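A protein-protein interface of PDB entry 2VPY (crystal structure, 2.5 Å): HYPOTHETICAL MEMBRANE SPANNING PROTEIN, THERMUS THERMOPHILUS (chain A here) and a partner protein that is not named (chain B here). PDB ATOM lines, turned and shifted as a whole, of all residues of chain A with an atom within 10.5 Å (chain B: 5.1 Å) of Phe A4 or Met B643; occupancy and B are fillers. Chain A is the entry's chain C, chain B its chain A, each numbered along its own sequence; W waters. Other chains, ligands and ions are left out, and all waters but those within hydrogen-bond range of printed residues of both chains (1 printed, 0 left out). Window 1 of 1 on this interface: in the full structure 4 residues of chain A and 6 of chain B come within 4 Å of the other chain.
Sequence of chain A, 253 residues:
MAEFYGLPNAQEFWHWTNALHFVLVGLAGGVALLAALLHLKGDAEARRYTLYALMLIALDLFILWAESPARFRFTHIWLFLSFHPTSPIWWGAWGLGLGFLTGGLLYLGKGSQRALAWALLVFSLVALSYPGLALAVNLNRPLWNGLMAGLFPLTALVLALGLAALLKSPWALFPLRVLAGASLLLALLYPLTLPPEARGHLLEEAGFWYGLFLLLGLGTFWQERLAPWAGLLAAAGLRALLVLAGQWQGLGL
Printed residues of chain B that touch a printed residue of chain A: Glu B642, Met B643 and Asp B644.
Hydrophobic or aromatic side chains of chain B within 4 Å of the printed part of chain A: Met B643.
Among the printed residues, no Asp or Glu carboxylate lies within 4 Å of a Lys or Arg side-chain nitrogen of the other chain.
The backbone carbonyl oxygen (O) of Met B643 is in hydrogen-bond range of the backbone NH (N) of Gly A6 (3.3 Å).
O of Phe A4 touches O of Met B643 (3.8 Å).
CD2 of Tyr A5 touches O of Met B643, at 3.2 Å.
CE2 of Tyr A5 touches CB of Asp B644 (3.9 Å).
Gly A6 touches Glu B642 (CA to O, 3.6 Å).
Water W1 lies within hydrogen-bond range of the backbone carbonyl oxygen (O) of Phe A4 and the backbone carbonyl oxygen (O) of Met B643.
Glu A3 touches none of the printed residues of chain B.
Of chain B, only Met B643 (3.8 Å) comes within 4 Å of Phe A4.
Of the printed residues of chain B, Tyr A5 touches Met B643 and Asp B644.
Printed residues of chain B within 4 Å of Gly A6: Glu B642 and Met B643.
Val B639 touches none of the printed residues of chain A.
Printed residues of chain A within 4 Å of Glu B642: Gly A6 (3.6 Å).
Of chain A, only Phe A4 (3.8 Å), Tyr A5 (3.2 Å) and Gly A6 (3.3 Å) come within 4 Å of Met B643.
Asp B644 touches just one residue of chain A: Tyr A5 (3.9 Å).
The nearest printed residue of chain B that does not touch Phe A4 is Asp B644 (5.6 Å).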
ATOM      1  N   ALA A   2     -19.656  -8.518   9.005  1.00  0.00           N
ATOM      2  CA  ALA A   2     -18.892  -9.754   9.288  1.00  0.00           C
ATOM      3  C   ALA A   2     -17.547  -9.692   8.517  1.00  0.00           C
ATOM      4  O   ALA A   2     -16.499  -9.893   9.131  1.00  0.00           O
ATOM      5  CB  ALA A   2     -19.730 -10.982   8.914  1.00  0.00           C
ATOM      6  N   GLU A   3     -17.573  -9.393   7.207  1.00  0.00           N
ATOM      7  CA  GLU A   3     -16.360  -9.226   6.356  1.00  0.00           C
ATOM      8  C   GLU A   3     -16.141  -7.743   6.001  1.00  0.00           C
ATOM      9  O   GLU A   3     -17.110  -7.025   5.787  1.00  0.00           O
ATOM     10  CB  GLU A   3     -16.496  -9.928   4.997  1.00  0.00           C
ATOM     11  CG  GLU A   3     -16.928 -11.346   5.055  1.00  0.00           C
ATOM     12  CD  GLU A   3     -15.829 -12.250   5.532  1.00  0.00           C
ATOM     13  OE1 GLU A   3     -14.942 -12.565   4.716  1.00  0.00           O
ATOM     14  OE2 GLU A   3     -15.847 -12.629   6.723  1.00  0.00           O
ATOM     15  N   PHE A   4     -14.891  -7.297   5.882  1.00  0.00           N
ATOM     16  CA  PHE A   4     -14.607  -5.901   5.505  1.00  0.00           C
ATOM     17  C   PHE A   4     -13.613  -5.743   4.361  1.00  0.00           C
ATOM     18  O   PHE A   4     -12.916  -6.677   4.020  1.00  0.00           O
ATOM     19  CB  PHE A   4     -13.956  -5.094   6.649  1.00  0.00           C
ATOM     20  CG  PHE A   4     -14.720  -5.074   7.922  1.00  0.00           C
ATOM     21  CD1 PHE A   4     -14.526  -6.068   8.870  1.00  0.00           C
ATOM     22  CD2 PHE A   4     -15.654  -4.066   8.170  1.00  0.00           C
ATOM     23  CE1 PHE A   4     -15.256  -6.070  10.062  1.00  0.00           C
ATOM     24  CE2 PHE A   4     -16.388  -4.048   9.347  1.00  0.00           C
ATOM     25  CZ  PHE A   4     -16.194  -5.058  10.301  1.00  0.00           C
ATOM     26  N   TYR A   5     -13.593  -4.540   3.773  1.00  0.00           N
ATOM     27  CA  TYR A   5     -12.556  -4.140   2.826  1.00  0.00           C
ATOM     28  C   TYR A   5     -12.059  -2.927   3.582  1.00  0.00           C
ATOM     29  O   TYR A   5     -12.767  -1.917   3.792  1.00  0.00           O
ATOM     30  CB  TYR A   5     -13.026  -3.813   1.430  1.00  0.00           C
ATOM     31  CG  TYR A   5     -13.302  -5.072   0.669  1.00  0.00           C
ATOM     32  CD1 TYR A   5     -14.578  -5.325   0.200  1.00  0.00           C
ATOM     33  CD2 TYR A   5     -12.312  -6.043   0.471  1.00  0.00           C
ATOM     34  CE1 TYR A   5     -14.885  -6.499  -0.441  1.00  0.00           C
ATOM     35  CE2 TYR A   5     -12.600  -7.238  -0.177  1.00  0.00           C
ATOM     36  CZ  TYR A   5     -13.904  -7.457  -0.634  1.00  0.00           C
ATOM     37  OH  TYR A   5     -14.239  -8.621  -1.295  1.00  0.00           O
ATOM     38  N   GLY A   6     -10.822  -3.086   4.022  1.00  0.00           N
ATOM     39  CA  GLY A   6     -10.217  -2.115   4.884  1.00  0.00           C
ATOM     40  C   GLY A   6     -10.766  -2.604   6.226  1.00  0.00           C
ATOM     41  O   GLY A   6     -11.182  -3.762   6.363  1.00  0.00           O
ATOM     42  N   LEU A   7     -10.820  -1.697   7.192  1.00  0.00           N
ATOM     43  CA  LEU A   7     -11.296  -1.956   8.557  1.00  0.00           C
ATOM     44  C   LEU A   7     -11.820  -0.693   9.257  1.00  0.00           C
ATOM     45  O   LEU A   7     -11.373   0.414   8.934  1.00  0.00           O
ATOM     46  CB  LEU A   7     -10.146  -2.421   9.438  1.00  0.00           C
ATOM     47  CG  LEU A   7      -9.503  -3.786   9.276  1.00  0.00           C
ATOM     48  CD1 LEU A   7      -8.147  -3.825  10.010  1.00  0.00           C
ATOM     49  CD2 LEU A   7     -10.493  -4.845   9.788  1.00  0.00           C
ATOM     50  N   PRO A   8     -12.789  -0.843  10.195  1.00  0.00           N
ATOM     51  CA  PRO A   8     -13.288   0.332  10.913  1.00  0.00           C
ATOM     52  C   PRO A   8     -12.168   0.607  11.914  1.00  0.00           C
ATOM     53  O   PRO A   8     -11.422  -0.312  12.264  1.00  0.00           O
ATOM     54  CB  PRO A   8     -14.528  -0.159  11.661  1.00  0.00           C
ATOM     55  CG  PRO A   8     -14.527  -1.630  11.524  1.00  0.00           C
ATOM     56  CD  PRO A   8     -13.744  -1.954  10.284  1.00  0.00           C
ATOM     57  N   ASN A   9     -12.065   1.843  12.387  1.00  0.00           N
ATOM     58  CA  ASN A   9     -11.055   2.234  13.365  1.00  0.00           C
ATOM     59  C   ASN A   9     -11.588   1.943  14.776  1.00  0.00           C
ATOM     60  O   ASN A   9     -11.911   2.863  15.538  1.00  0.00           O
ATOM     61  CB  ASN A   9     -10.764   3.724  13.208  1.00  0.00           C
ATOM     62  CG  ASN A   9     -10.334   4.075  11.805  1.00  0.00           C
ATOM     63  OD1 ASN A   9     -11.028   4.781  11.076  1.00  0.00           O
ATOM     64  ND2 ASN A   9      -9.186   3.568  11.414  1.00  0.00           N
ATOM     65  N   ALA A  10     -11.669   0.660  15.118  1.00  0.00           N
ATOM     66  CA  ALA A  10     -12.212   0.208  16.391  1.00  0.00           C
ATOM     67  C   ALA A  10     -11.200  -0.310  17.390  1.00  0.00           C
ATOM     68  O   ALA A  10     -11.548  -1.061  18.299  1.00  0.00           O
ATOM     69  CB  ALA A  10     -13.283  -0.867  16.154  1.00  0.00           C
ATOM     70  N   VAL B 628     -10.915  -6.173  -5.479  1.00  0.00           N
ATOM     71  CA  VAL B 628      -9.767  -5.326  -5.178  1.00  0.00           C
ATOM     72  C   VAL B 628      -8.365  -5.814  -5.598  1.00  0.00           C
ATOM     73  O   VAL B 628      -7.372  -5.076  -5.532  1.00  0.00           O
ATOM     74  CB  VAL B 628      -9.846  -5.113  -3.618  1.00  0.00           C
ATOM     75  CG1 VAL B 628      -8.544  -4.739  -3.037  1.00  0.00           C
ATOM     76  CG2 VAL B 628     -10.945  -4.061  -3.280  1.00  0.00           C
ATOM     77  N   VAL B 639      -1.721  -0.655  -0.714  1.00  0.00           N
ATOM     78  CA  VAL B 639      -3.034  -0.003  -0.702  1.00  0.00           C
ATOM     79  C   VAL B 639      -4.150  -1.050  -0.904  1.00  0.00           C
ATOM     80  O   VAL B 639      -5.235  -0.960  -0.339  1.00  0.00           O
ATOM     81  CB  VAL B 639      -3.156   1.066  -1.849  1.00  0.00           C
ATOM     82  CG1 VAL B 639      -4.598   1.572  -1.974  1.00  0.00           C
ATOM     83  CG2 VAL B 639      -2.187   2.214  -1.574  1.00  0.00           C
ATOM     84  N   LEU B 640      -3.851  -2.057  -1.708  1.00  0.00           N
ATOM     85  CA  LEU B 640      -4.810  -3.086  -2.029  1.00  0.00           C
ATOM     86  C   LEU B 640      -4.786  -4.289  -1.083  1.00  0.00           C
ATOM     87  O   LEU B 640      -5.830  -4.909  -0.797  1.00  0.00           O
ATOM     88  CB  LEU B 640      -4.656  -3.506  -3.496  1.00  0.00           C
ATOM     89  CG  LEU B 640      -5.021  -2.402  -4.539  1.00  0.00           C
ATOM     90  CD1 LEU B 640      -4.680  -2.890  -5.954  1.00  0.00           C
ATOM     91  CD2 LEU B 640      -6.516  -2.019  -4.430  1.00  0.00           C
ATOM     92  N   MET B 641      -3.612  -4.619  -0.561  1.00  0.00           N
ATOM     93  CA  MET B 641      -3.535  -5.723   0.392  1.00  0.00           C
ATOM     94  C   MET B 641      -4.194  -5.302   1.729  1.00  0.00           C
ATOM     95  O   MET B 641      -4.706  -6.130   2.479  1.00  0.00           O
ATOM     96  CB  MET B 641      -2.075  -6.135   0.620  1.00  0.00           C
ATOM     97  CG  MET B 641      -1.556  -7.194  -0.359  1.00  0.00           C
ATOM     98  SD  MET B 641      -2.482  -8.780  -0.243  1.00  0.00           S
ATOM     99  CE  MET B 641      -1.798  -9.458   1.281  1.00  0.00           C
ATOM    100  N   GLU B 642      -4.180  -3.999   1.991  1.00  0.00           N
ATOM    101  CA  GLU B 642      -4.748  -3.434   3.208  1.00  0.00           C
ATOM    102  C   GLU B 642      -6.283  -3.463   3.170  1.00  0.00           C
ATOM    103  O   GLU B 642      -6.948  -3.350   4.203  1.00  0.00           O
ATOM    104  CB  GLU B 642      -4.216  -2.021   3.374  1.00  0.00           C
ATOM    105  CG  GLU B 642      -4.445  -1.385   4.672  1.00  0.00           C
ATOM    106  CD  GLU B 642      -3.684  -0.109   4.743  1.00  0.00           C
ATOM    107  OE1 GLU B 642      -4.005   0.794   3.942  1.00  0.00           O
ATOM    108  OE2 GLU B 642      -2.737  -0.027   5.543  1.00  0.00           O
ATOM    109  N   MET B 643      -6.827  -3.594   1.962  1.00  0.00           N
ATOM    110  CA  MET B 643      -8.268  -3.728   1.777  1.00  0.00           C
ATOM    111  C   MET B 643      -8.598  -5.238   1.824  1.00  0.00           C
ATOM    112  O   MET B 643      -9.673  -5.604   2.250  1.00  0.00           O
ATOM    113  CB  MET B 643      -8.742  -3.197   0.419  1.00  0.00           C
ATOM    114  CG  MET B 643      -8.517  -1.719   0.213  1.00  0.00           C
ATOM    115  SD  MET B 643      -9.597  -0.747   1.262  1.00  0.00           S
ATOM    116  CE  MET B 643      -8.959   0.954   0.927  1.00  0.00           C
ATOM    117  N   ASP B 644      -7.663  -6.095   1.400  1.00  0.00           N
ATOM    118  CA  ASP B 644      -7.897  -7.560   1.340  1.00  0.00           C
ATOM    119  C   ASP B 644      -6.549  -8.262   1.360  1.00  0.00           C
ATOM    120  O   ASP B 644      -5.947  -8.571   0.291  1.00  0.00           O
ATOM    121  CB  ASP B 644      -8.720  -7.870   0.084  1.00  0.00           C
ATOM    122  CG  ASP B 644      -9.214  -9.309   0.038  1.00  0.00           C
ATOM    123  OD1 ASP B 644      -9.370  -9.924   1.112  1.00  0.00           O
ATOM    124  OD2 ASP B 644      -9.474  -9.804  -1.079  1.00  0.00           O
ATOM    125  N   PRO B 645      -6.048  -8.568   2.585  1.00  0.00           N
ATOM    126  CA  PRO B 645      -4.795  -9.210   2.975  1.00  0.00           C
ATOM    127  C   PRO B 645      -4.730 -10.722   2.868  1.00  0.00           C
ATOM    128  O   PRO B 645      -3.674 -11.308   3.030  1.00  0.00           O
ATOM    129  CB  PRO B 645      -4.598  -8.705   4.402  1.00  0.00           C
ATOM    130  CG  PRO B 645      -6.020  -8.301   4.883  1.00  0.00           C
ATOM    131  CD  PRO B 645      -6.952  -8.652   3.729  1.00  0.00           C
HETATM  132  O   HOH W   1     -10.557  -7.614   3.954  1.00  0.00           O
